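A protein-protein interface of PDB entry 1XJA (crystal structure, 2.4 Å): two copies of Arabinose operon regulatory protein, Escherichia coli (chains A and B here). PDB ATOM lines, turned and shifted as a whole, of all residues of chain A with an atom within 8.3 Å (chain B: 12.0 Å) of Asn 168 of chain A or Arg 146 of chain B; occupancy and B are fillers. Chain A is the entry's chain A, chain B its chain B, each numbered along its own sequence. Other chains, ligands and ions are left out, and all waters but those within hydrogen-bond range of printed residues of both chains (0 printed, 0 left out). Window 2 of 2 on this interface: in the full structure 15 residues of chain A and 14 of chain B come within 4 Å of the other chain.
Of the 12 printed residues of chain A, 6 touch a printed residue of chain B. Printed residues of chain A that touch a printed residue of chain B: Trp 107, Leu 161, Arg 162, Met 164, Glu 165 and Asn 168. Hydrophobic or aromatic side chains of chain A that line the printed part of chain B: Trp 107, Leu 161 and Met 164. Of the 22 printed residues of chain B, 5 touch a printed residue of chain A. Printed residues of chain B that touch a printed residue of chain A: Arg 146, Tyr 147, Ser 148, Leu 150 and Leu 151. Hydrophobic or aromatic side chains of chain B within 4 Å of the printed part of chain A: Tyr 147, Leu 150 and Leu 151. Among the printed residues, 8 pairs touch across the chains. Among the printed residues, no Asp or Glu carboxylate lies within 4 Å of a Lys or Arg side-chain nitrogen of the other chain.
The guanidinium group (NH1) of Arg 163 of chain A lies within hydrogen-bond range of the side-chain sulfur (SD) of Met 164 of chain A, 3.8 Å away. O of Gly 145 of chain B lies within hydrogen-bond range of OG of Ser 148 of chain B, 2.8 Å away.
No position is printed for both chains. Of the 8 pairs that touch across the chains among the printed residues, none has its exchanged pair printed and touching as well.
NE1 of Trp 107 of chain A touches CE1 of Tyr 147 of chain B (3.9 Å). Trp 107 of chain A touches Leu 150 of chain B (CZ2 to CD1, 3.8 Å). Leu 150 of chain B touches Leu 161 of chain A (O to CD1, 3.6 Å). Arg 162 of chain A touches Leu 151 of chain B (NH1 to CD1, 3.6 Å). Met 164 of chain A touches Tyr 147 of chain B. Arg 146 of chain B touches Asn 168 of chain A.
The side-chain carboxylate of Glu 165 of chain A sits close to the backbone NH of Tyr 147 of chain B, 3.1 Å away. OE1 of Glu 165 of chain A lies within hydrogen-bond range of N of Ser 148 of chain B.
Printed residues of chain B within 4 Å of Trp 107 of chain A: Tyr 147 (3.9 Å) and Leu 150 (3.8 Å). Printed residues of chain B within 4 Å of Leu 161 of chain A: Leu 150 (3.6 Å). Met 164 of chain A touches just one residue of chain B: Tyr 147. Glu 165 of chain A touches just these residues of chain B: Tyr 147 (2.9 Å) and Ser 148 (3.5 Å). No residue of chain B comes within 4 Å of Ala 166 of chain A. Asn 168 of chain A touches just one residue of chain B: Arg 146 (3.8 Å). No residue of chain B comes within 4 Å of Glu 169 of chain A. Ala 140 of chain B touches none of the printed residues of chain A. Of chain A, only Asn 168 (3.8 Å) comes within 4 Å of Arg 146 of chain B. Of the printed residues of chain A, Tyr 147 of chain B touches Trp 107 (3.9 Å), Met 164 (3.1 Å) and Glu 165 (2.9 Å). Of the printed residues of chain A, Ser 148 of chain B touches Glu 165. Printed residues of chain A within 4 Å of Leu 151 of chain B: Arg 162 (3.6 Å). The nearest residue of chain B that does not touch Asn 168 of chain A is Tyr 147 of chain B (4.3 Å).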
ATOM      1  N   TRP A 107       9.639   9.118  -7.752  1.00  0.00           N
ATOM      2  CA  TRP A 107       9.945  10.206  -8.678  1.00  0.00           C
ATOM      3  C   TRP A 107       9.478  11.588  -8.204  1.00  0.00           C
ATOM      4  O   TRP A 107       9.508  12.554  -8.973  1.00  0.00           O
ATOM      5  CB  TRP A 107       9.326   9.904 -10.045  1.00  0.00           C
ATOM      6  CG  TRP A 107       9.406   8.461 -10.439  1.00  0.00           C
ATOM      7  CD1 TRP A 107      10.455   7.611 -10.243  1.00  0.00           C
ATOM      8  CD2 TRP A 107       8.403   7.702 -11.130  1.00  0.00           C
ATOM      9  NE1 TRP A 107      10.167   6.372 -10.767  1.00  0.00           N
ATOM     10  CE2 TRP A 107       8.915   6.402 -11.316  1.00  0.00           C
ATOM     11  CE3 TRP A 107       7.122   7.999 -11.609  1.00  0.00           C
ATOM     12  CZ2 TRP A 107       8.196   5.405 -11.960  1.00  0.00           C
ATOM     13  CZ3 TRP A 107       6.409   7.008 -12.251  1.00  0.00           C
ATOM     14  CH2 TRP A 107       6.944   5.724 -12.420  1.00  0.00           C
ATOM     15  N   LEU A 161       8.754  11.120 -15.443  1.00  0.00           N
ATOM     16  CA  LEU A 161       9.677  10.124 -15.974  1.00  0.00           C
ATOM     17  C   LEU A 161      10.775  10.750 -16.833  1.00  0.00           C
ATOM     18  O   LEU A 161      11.925  10.280 -16.829  1.00  0.00           O
ATOM     19  CB  LEU A 161       8.918   9.070 -16.783  1.00  0.00           C
ATOM     20  CG  LEU A 161       8.053   8.140 -15.931  1.00  0.00           C
ATOM     21  CD1 LEU A 161       7.285   7.164 -16.816  1.00  0.00           C
ATOM     22  CD2 LEU A 161       8.950   7.390 -14.961  1.00  0.00           C
ATOM     23  N   ARG A 162      10.425  11.801 -17.573  1.00  0.00           N
ATOM     24  CA  ARG A 162      11.406  12.472 -18.413  1.00  0.00           C
ATOM     25  C   ARG A 162      12.460  13.066 -17.495  1.00  0.00           C
ATOM     26  O   ARG A 162      13.651  13.055 -17.808  1.00  0.00           O
ATOM     27  CB  ARG A 162      10.759  13.591 -19.231  1.00  0.00           C
ATOM     28  CG  ARG A 162       9.752  13.131 -20.266  1.00  0.00           C
ATOM     29  CD  ARG A 162      10.426  12.416 -21.402  1.00  0.00           C
ATOM     30  NE  ARG A 162       9.487  12.033 -22.456  1.00  0.00           N
ATOM     31  CZ  ARG A 162       9.807  11.281 -23.506  1.00  0.00           C
ATOM     32  NH1 ARG A 162      11.045  10.828 -23.648  1.00  0.00           N
ATOM     33  NH2 ARG A 162       8.888  10.968 -24.407  1.00  0.00           N
ATOM     34  N   ARG A 163      12.014  13.580 -16.356  1.00  0.00           N
ATOM     35  CA  ARG A 163      12.932  14.175 -15.400  1.00  0.00           C
ATOM     36  C   ARG A 163      13.850  13.127 -14.799  1.00  0.00           C
ATOM     37  O   ARG A 163      15.049  13.358 -14.672  1.00  0.00           O
ATOM     38  CB  ARG A 163      12.172  14.894 -14.281  1.00  0.00           C
ATOM     39  CG  ARG A 163      13.079  15.356 -13.140  1.00  0.00           C
ATOM     40  CD  ARG A 163      12.343  16.179 -12.088  1.00  0.00           C
ATOM     41  NE  ARG A 163      13.231  16.472 -10.966  1.00  0.00           N
ATOM     42  CZ  ARG A 163      13.653  15.557 -10.094  1.00  0.00           C
ATOM     43  NH1 ARG A 163      13.258  14.292 -10.202  1.00  0.00           N
ATOM     44  NH2 ARG A 163      14.497  15.897  -9.134  1.00  0.00           N
ATOM     45  N   MET A 164      13.298  11.979 -14.419  1.00  0.00           N
ATOM     46  CA  MET A 164      14.125  10.920 -13.842  1.00  0.00           C
ATOM     47  C   MET A 164      15.143  10.497 -14.892  1.00  0.00           C
ATOM     48  O   MET A 164      16.329  10.396 -14.610  1.00  0.00           O
ATOM     49  CB  MET A 164      13.282   9.707 -13.438  1.00  0.00           C
ATOM     50  CG  MET A 164      12.227   9.989 -12.390  1.00  0.00           C
ATOM     51  SD  MET A 164      12.932  10.584 -10.850  1.00  0.00           S
ATOM     52  CE  MET A 164      13.915   9.136 -10.336  1.00  0.00           C
ATOM     53  N   GLU A 165      14.672  10.256 -16.112  1.00  0.00           N
ATOM     54  CA  GLU A 165      15.561   9.849 -17.193  1.00  0.00           C
ATOM     55  C   GLU A 165      16.625  10.916 -17.450  1.00  0.00           C
ATOM     56  O   GLU A 165      17.799  10.596 -17.641  1.00  0.00           O
ATOM     57  CB  GLU A 165      14.768   9.600 -18.479  1.00  0.00           C
ATOM     58  CG  GLU A 165      15.577   8.919 -19.568  1.00  0.00           C
ATOM     59  CD  GLU A 165      15.978   7.500 -19.179  1.00  0.00           C
ATOM     60  OE1 GLU A 165      15.154   6.569 -19.343  1.00  0.00           O
ATOM     61  OE2 GLU A 165      17.116   7.315 -18.693  1.00  0.00           O
ATOM     62  N   ALA A 166      16.219  12.181 -17.444  1.00  0.00           N
ATOM     63  CA  ALA A 166      17.154  13.279 -17.691  1.00  0.00           C
ATOM     64  C   ALA A 166      18.224  13.411 -16.615  1.00  0.00           C
ATOM     65  O   ALA A 166      19.397  13.564 -16.927  1.00  0.00           O
ATOM     66  CB  ALA A 166      16.394  14.592 -17.835  1.00  0.00           C
ATOM     67  N   ILE A 167      17.824  13.367 -15.349  1.00  0.00           N
ATOM     68  CA  ILE A 167      18.784  13.467 -14.253  1.00  0.00           C
ATOM     69  C   ILE A 167      19.715  12.269 -14.354  1.00  0.00           C
ATOM     70  O   ILE A 167      20.934  12.383 -14.221  1.00  0.00           O
ATOM     71  CB  ILE A 167      18.106  13.387 -12.868  1.00  0.00           C
ATOM     72  CG1 ILE A 167      16.990  14.433 -12.741  1.00  0.00           C
ATOM     73  CG2 ILE A 167      19.155  13.569 -11.779  1.00  0.00           C
ATOM     74  CD1 ILE A 167      17.439  15.836 -12.407  1.00  0.00           C
ATOM     75  N   ASN A 168      19.118  11.114 -14.602  1.00  0.00           N
ATOM     76  CA  ASN A 168      19.858   9.870 -14.698  1.00  0.00           C
ATOM     77  C   ASN A 168      21.070   9.864 -15.625  1.00  0.00           C
ATOM     78  O   ASN A 168      21.973   9.054 -15.445  1.00  0.00           O
ATOM     79  CB  ASN A 168      18.926   8.736 -15.115  1.00  0.00           C
ATOM     80  CG  ASN A 168      19.610   7.382 -15.071  1.00  0.00           C
ATOM     81  OD1 ASN A 168      19.377   6.522 -15.926  1.00  0.00           O
ATOM     82  ND2 ASN A 168      20.455   7.182 -14.066  1.00  0.00           N
ATOM     83  N   GLU A 169      21.113  10.741 -16.618  1.00  0.00           N
ATOM     84  CA  GLU A 169      22.261  10.712 -17.511  1.00  0.00           C
ATOM     85  C   GLU A 169      23.037  12.000 -17.614  1.00  0.00           C
ATOM     86  O   GLU A 169      24.083  12.044 -18.259  1.00  0.00           O
ATOM     87  CB  GLU A 169      21.836  10.266 -18.901  1.00  0.00           C
ATOM     88  CG  GLU A 169      20.879  11.199 -19.585  1.00  0.00           C
ATOM     89  CD  GLU A 169      20.192  10.514 -20.740  1.00  0.00           C
ATOM     90  OE1 GLU A 169      19.503  11.201 -21.526  1.00  0.00           O
ATOM     91  OE2 GLU A 169      20.343   9.276 -20.853  1.00  0.00           O
ATOM     92  N   SER A 170      22.532  13.051 -16.983  1.00  0.00           N
ATOM     93  CA  SER A 170      23.232  14.325 -17.008  1.00  0.00           C
ATOM     94  C   SER A 170      24.542  14.146 -16.258  1.00  0.00           C
ATOM     95  O   SER A 170      24.874  13.048 -15.805  1.00  0.00           O
ATOM     96  CB  SER A 170      22.401  15.413 -16.325  1.00  0.00           C
ATOM     97  OG  SER A 170      22.171  15.097 -14.963  1.00  0.00           O
ATOM     98  N   LEU A 171      25.293  15.230 -16.139  1.00  0.00           N
ATOM     99  CA  LEU A 171      26.547  15.179 -15.420  1.00  0.00           C
ATOM    100  C   LEU A 171      26.441  16.022 -14.170  1.00  0.00           C
ATOM    101  O   LEU A 171      25.381  16.571 -13.837  1.00  0.00           O
ATOM    102  CB  LEU A 171      27.691  15.676 -16.285  1.00  0.00           C
ATOM    103  N   PHE B  15      16.234  -8.778 -18.291  1.00  0.00           N
ATOM    104  CA  PHE B  15      15.410  -8.232 -19.403  1.00  0.00           C
ATOM    105  C   PHE B  15      13.977  -7.980 -18.921  1.00  0.00           C
ATOM    106  O   PHE B  15      13.486  -8.630 -17.993  1.00  0.00           O
ATOM    107  CB  PHE B  15      15.420  -9.213 -20.587  1.00  0.00           C
ATOM    108  CG  PHE B  15      14.766  -8.680 -21.847  1.00  0.00           C
ATOM    109  CD1 PHE B  15      14.124  -7.446 -21.860  1.00  0.00           C
ATOM    110  CD2 PHE B  15      14.760  -9.441 -23.011  1.00  0.00           C
ATOM    111  CE1 PHE B  15      13.482  -6.972 -22.996  1.00  0.00           C
ATOM    112  CE2 PHE B  15      14.122  -8.977 -24.162  1.00  0.00           C
ATOM    113  CZ  PHE B  15      13.478  -7.736 -24.150  1.00  0.00           C
ATOM    114  N   ASN B  16      13.342  -7.007 -19.572  1.00  0.00           N
ATOM    115  CA  ASN B  16      11.974  -6.547 -19.328  1.00  0.00           C
ATOM    116  C   ASN B  16      10.966  -7.585 -18.855  1.00  0.00           C
ATOM    117  O   ASN B  16      10.929  -8.719 -19.342  1.00  0.00           O
ATOM    118  CB  ASN B  16      11.418  -5.896 -20.602  1.00  0.00           C
ATOM    119  CG  ASN B  16      12.260  -4.725 -21.084  1.00  0.00           C
ATOM    120  OD1 ASN B  16      13.463  -4.663 -20.835  1.00  0.00           O
ATOM    121  ND2 ASN B  16      11.631  -3.799 -21.795  1.00  0.00           N
ATOM    122  N   ALA B  17      10.124  -7.178 -17.916  1.00  0.00           N
ATOM    123  CA  ALA B  17       9.100  -8.069 -17.411  1.00  0.00           C
ATOM    124  C   ALA B  17       7.748  -7.368 -17.501  1.00  0.00           C
ATOM    125  O   ALA B  17       6.817  -7.715 -16.772  1.00  0.00           O
ATOM    126  CB  ALA B  17       9.407  -8.455 -15.973  1.00  0.00           C
ATOM    127  N   HIS B  18       7.636  -6.390 -18.399  1.00  0.00           N
ATOM    128  CA  HIS B  18       6.386  -5.652 -18.546  1.00  0.00           C
ATOM    129  C   HIS B  18       6.010  -5.233 -19.954  1.00  0.00           C
ATOM    130  O   HIS B  18       4.849  -5.354 -20.359  1.00  0.00           O
ATOM    131  CB  HIS B  18       6.411  -4.440 -17.627  1.00  0.00           C
ATOM    132  CG  HIS B  18       6.191  -4.793 -16.194  1.00  0.00           C
ATOM    133  ND1 HIS B  18       4.940  -5.070 -15.688  1.00  0.00           N
ATOM    134  CD2 HIS B  18       7.066  -5.013 -15.184  1.00  0.00           C
ATOM    135  CE1 HIS B  18       5.052  -5.446 -14.427  1.00  0.00           C
ATOM    136  NE2 HIS B  18       6.332  -5.422 -14.097  1.00  0.00           N
ATOM    137  N   LEU B  19       6.978  -4.735 -20.706  1.00  0.00           N
ATOM    138  CA  LEU B  19       6.678  -4.331 -22.060  1.00  0.00           C
ATOM    139  C   LEU B  19       7.860  -4.557 -22.977  1.00  0.00           C
ATOM    140  O   LEU B  19       8.988  -4.184 -22.668  1.00  0.00           O
ATOM    141  CB  LEU B  19       6.240  -2.866 -22.092  1.00  0.00           C
ATOM    142  CG  LEU B  19       5.752  -2.324 -23.438  1.00  0.00           C
ATOM    143  CD1 LEU B  19       4.876  -1.112 -23.203  1.00  0.00           C
ATOM    144  CD2 LEU B  19       6.934  -1.982 -24.334  1.00  0.00           C
ATOM    145  N   ARG B 101      -1.494  -2.491 -16.857  1.00  0.00           N
ATOM    146  CA  ARG B 101      -1.632  -2.045 -15.469  1.00  0.00           C
ATOM    147  C   ARG B 101      -3.077  -2.331 -15.112  1.00  0.00           C
ATOM    148  O   ARG B 101      -3.946  -2.265 -15.978  1.00  0.00           O
ATOM    149  CB  ARG B 101      -1.360  -0.540 -15.342  1.00  0.00           C
ATOM    150  CG  ARG B 101       0.093  -0.112 -15.506  1.00  0.00           C
ATOM    151  CD  ARG B 101       0.202   1.378 -15.286  1.00  0.00           C
ATOM    152  NE  ARG B 101       1.559   1.889 -15.453  1.00  0.00           N
ATOM    153  CZ  ARG B 101       2.585   1.579 -14.671  1.00  0.00           C
ATOM    154  NH1 ARG B 101       2.424   0.748 -13.651  1.00  0.00           N
ATOM    155  NH2 ARG B 101       3.777   2.113 -14.906  1.00  0.00           N
ATOM    156  N   ASN B 139      10.349   2.668 -29.780  1.00  0.00           N
ATOM    157  CA  ASN B 139      11.675   3.162 -29.455  1.00  0.00           C
ATOM    158  C   ASN B 139      11.927   3.101 -27.968  1.00  0.00           C
ATOM    159  O   ASN B 139      12.997   2.691 -27.535  1.00  0.00           O
ATOM    160  CB  ASN B 139      11.831   4.589 -29.967  1.00  0.00           C
ATOM    161  CG  ASN B 139      11.632   4.684 -31.468  1.00  0.00           C
ATOM    162  OD1 ASN B 139      11.516   5.779 -32.029  1.00  0.00           O
ATOM    163  ND2 ASN B 139      11.593   3.527 -32.133  1.00  0.00           N
ATOM    164  N   ALA B 140      10.940   3.505 -27.182  1.00  0.00           N
ATOM    165  CA  ALA B 140      11.083   3.471 -25.736  1.00  0.00           C
ATOM    166  C   ALA B 140      11.285   2.024 -25.322  1.00  0.00           C
ATOM    167  O   ALA B 140      12.181   1.709 -24.538  1.00  0.00           O
ATOM    168  CB  ALA B 140       9.844   4.032 -25.074  1.00  0.00           C
ATOM    169  N   GLY B 141      10.451   1.149 -25.872  1.00  0.00           N
ATOM    170  CA  GLY B 141      10.534  -0.265 -25.555  1.00  0.00           C
ATOM    171  C   GLY B 141      11.861  -0.927 -25.889  1.00  0.00           C
ATOM    172  O   GLY B 141      12.218  -1.945 -25.291  1.00  0.00           O
ATOM    173  N   GLN B 142      12.599  -0.353 -26.834  1.00  0.00           N
ATOM    174  CA  GLN B 142      13.884  -0.919 -27.234  1.00  0.00           C
ATOM    175  C   GLN B 142      15.075  -0.128 -26.707  1.00  0.00           C
ATOM    176  O   GLN B 142      16.227  -0.467 -26.988  1.00  0.00           O
ATOM    177  CB  GLN B 142      13.962  -1.007 -28.759  1.00  0.00           C
ATOM    178  CG  GLN B 142      12.912  -1.910 -29.373  1.00  0.00           C
ATOM    179  CD  GLN B 142      13.100  -2.080 -30.862  1.00  0.00           C
ATOM    180  OE1 GLN B 142      13.109  -1.104 -31.615  1.00  0.00           O
ATOM    181  NE2 GLN B 142      13.255  -3.325 -31.299  1.00  0.00           N
ATOM    182  N   GLY B 143      14.794   0.926 -25.946  1.00  0.00           N
ATOM    183  CA  GLY B 143      15.862   1.734 -25.390  1.00  0.00           C
ATOM    184  C   GLY B 143      16.610   0.997 -24.292  1.00  0.00           C
ATOM    185  O   GLY B 143      16.092   0.044 -23.704  1.00  0.00           O
ATOM    186  N   GLU B 144      17.834   1.435 -24.015  1.00  0.00           N
ATOM    187  CA  GLU B 144      18.644   0.804 -22.981  1.00  0.00           C
ATOM    188  C   GLU B 144      18.514   1.560 -21.663  1.00  0.00           C
ATOM    189  O   GLU B 144      18.843   1.033 -20.600  1.00  0.00           O
ATOM    190  CB  GLU B 144      20.101   0.756 -23.419  1.00  0.00           C
ATOM    191  N   GLY B 145      18.023   2.793 -21.747  1.00  0.00           N
ATOM    192  CA  GLY B 145      17.850   3.617 -20.565  1.00  0.00           C
ATOM    193  C   GLY B 145      17.122   2.918 -19.432  1.00  0.00           C
ATOM    194  O   GLY B 145      16.210   2.126 -19.660  1.00  0.00           O
ATOM    195  N   ARG B 146      17.529   3.217 -18.204  1.00  0.00           N
ATOM    196  CA  ARG B 146      16.920   2.623 -17.022  1.00  0.00           C
ATOM    197  C   ARG B 146      15.421   2.914 -16.947  1.00  0.00           C
ATOM    198  O   ARG B 146      14.655   2.124 -16.393  1.00  0.00           O
ATOM    199  CB  ARG B 146      17.606   3.152 -15.765  1.00  0.00           C
ATOM    200  CG  ARG B 146      16.946   2.687 -14.492  1.00  0.00           C
ATOM    201  CD  ARG B 146      16.659   3.866 -13.596  1.00  0.00           C
ATOM    202  NE  ARG B 146      17.790   4.242 -12.752  1.00  0.00           N
ATOM    203  CZ  ARG B 146      18.075   3.663 -11.590  1.00  0.00           C
ATOM    204  NH1 ARG B 146      17.307   2.681 -11.134  1.00  0.00           N
ATOM    205  NH2 ARG B 146      19.119   4.075 -10.881  1.00  0.00           N
ATOM    206  N   TYR B 147      15.006   4.047 -17.508  1.00  0.00           N
ATOM    207  CA  TYR B 147      13.596   4.426 -17.493  1.00  0.00           C
ATOM    208  C   TYR B 147      12.893   4.197 -18.829  1.00  0.00           C
ATOM    209  O   TYR B 147      11.754   4.612 -19.011  1.00  0.00           O
ATOM    210  CB  TYR B 147      13.456   5.889 -17.069  1.00  0.00           C
ATOM    211  CG  TYR B 147      13.765   6.096 -15.612  1.00  0.00           C
ATOM    212  CD1 TYR B 147      12.847   5.739 -14.630  1.00  0.00           C
ATOM    213  CD2 TYR B 147      15.009   6.579 -15.208  1.00  0.00           C
ATOM    214  CE1 TYR B 147      13.161   5.853 -13.280  1.00  0.00           C
ATOM    215  CE2 TYR B 147      15.337   6.694 -13.862  1.00  0.00           C
ATOM    216  CZ  TYR B 147      14.410   6.327 -12.903  1.00  0.00           C
ATOM    217  OH  TYR B 147      14.743   6.412 -11.575  1.00  0.00           O
ATOM    218  N   SER B 148      13.576   3.512 -19.742  1.00  0.00           N
ATOM    219  CA  SER B 148      13.044   3.224 -21.071  1.00  0.00           C
ATOM    220  C   SER B 148      11.740   2.451 -21.064  1.00  0.00           C
ATOM    221  O   SER B 148      10.793   2.821 -21.747  1.00  0.00           O
ATOM    222  CB  SER B 148      14.069   2.438 -21.896  1.00  0.00           C
ATOM    223  OG  SER B 148      15.271   3.168 -22.038  1.00  0.00           O
ATOM    224  N   GLU B 149      11.693   1.370 -20.301  1.00  0.00           N
ATOM    225  CA  GLU B 149      10.488   0.556 -20.249  1.00  0.00           C
ATOM    226  C   GLU B 149       9.313   1.316 -19.644  1.00  0.00           C
ATOM    227  O   GLU B 149       8.181   1.217 -20.130  1.00  0.00           O
ATOM    228  CB  GLU B 149      10.757  -0.736 -19.466  1.00  0.00           C
ATOM    229  CG  GLU B 149       9.538  -1.642 -19.334  1.00  0.00           C
ATOM    230  CD  GLU B 149       9.862  -2.941 -18.640  1.00  0.00           C
ATOM    231  OE1 GLU B 149      10.630  -2.907 -17.652  1.00  0.00           O
ATOM    232  OE2 GLU B 149       9.341  -3.991 -19.075  1.00  0.00           O
ATOM    233  N   LEU B 150       9.580   2.080 -18.589  1.00  0.00           N
ATOM    234  CA  LEU B 150       8.530   2.861 -17.940  1.00  0.00           C
ATOM    235  C   LEU B 150       7.981   3.921 -18.893  1.00  0.00           C
ATOM    236  O   LEU B 150       6.802   4.271 -18.837  1.00  0.00           O
ATOM    237  CB  LEU B 150       9.074   3.517 -16.674  1.00  0.00           C
ATOM    238  CG  LEU B 150       9.384   2.540 -15.534  1.00  0.00           C
ATOM    239  CD1 LEU B 150      10.174   3.248 -14.448  1.00  0.00           C
ATOM    240  CD2 LEU B 150       8.089   1.963 -14.982  1.00  0.00           C
ATOM    241  N   LEU B 151       8.832   4.433 -19.775  1.00  0.00           N
ATOM    242  CA  LEU B 151       8.385   5.436 -20.734  1.00  0.00           C
ATOM    243  C   LEU B 151       7.474   4.790 -21.766  1.00  0.00           C
ATOM    244  O   LEU B 151       6.425   5.333 -22.110  1.00  0.00           O
ATOM    245  CB  LEU B 151       9.578   6.088 -21.442  1.00  0.00           C
ATOM    246  CG  LEU B 151      10.102   7.398 -20.853  1.00  0.00           C
ATOM    247  CD1 LEU B 151      11.326   7.858 -21.632  1.00  0.00           C
ATOM    248  CD2 LEU B 151       9.002   8.458 -20.922  1.00  0.00           C
ATOM    249  N   ALA B 152       7.882   3.624 -22.254  1.00  0.00           N
ATOM    250  CA  ALA B 152       7.105   2.893 -23.247  1.00  0.00           C
ATOM    251  C   ALA B 152       5.734   2.580 -22.665  1.00  0.00           C
ATOM    252  O   ALA B 152       4.716   2.727 -23.343  1.00  0.00           O
ATOM    253  CB  ALA B 152       7.823   1.608 -23.630  1.00  0.00           C
ATOM    254  N   ILE B 153       5.720   2.155 -21.402  1.00  0.00           N
ATOM    255  CA  ILE B 153       4.478   1.837 -20.712  1.00  0.00           C
ATOM    256  C   ILE B 153       3.599   3.074 -20.667  1.00  0.00           C
ATOM    257  O   ILE B 153       2.402   3.024 -20.973  1.00  0.00           O
ATOM    258  CB  ILE B 153       4.754   1.342 -19.270  1.00  0.00           C
ATOM    259  CG1 ILE B 153       5.409  -0.039 -19.326  1.00  0.00           C
ATOM    260  CG2 ILE B 153       3.460   1.285 -18.469  1.00  0.00           C
ATOM    261  CD1 ILE B 153       5.661  -0.666 -17.978  1.00  0.00           C
ATOM    262  N   ASN B 154       4.205   4.190 -20.284  1.00  0.00           N
ATOM    263  CA  ASN B 154       3.501   5.460 -20.202  1.00  0.00           C
ATOM    264  C   ASN B 154       2.933   5.867 -21.556  1.00  0.00           C
ATOM    265  O   ASN B 154       1.778   6.292 -21.662  1.00  0.00           O
ATOM    266  CB  ASN B 154       4.453   6.552 -19.737  1.00  0.00           C
ATOM    267  CG  ASN B 154       3.813   7.910 -19.755  1.00  0.00           C
ATOM    268  OD1 ASN B 154       2.990   8.228 -18.897  1.00  0.00           O
ATOM    269  ND2 ASN B 154       4.162   8.711 -20.745  1.00  0.00           N
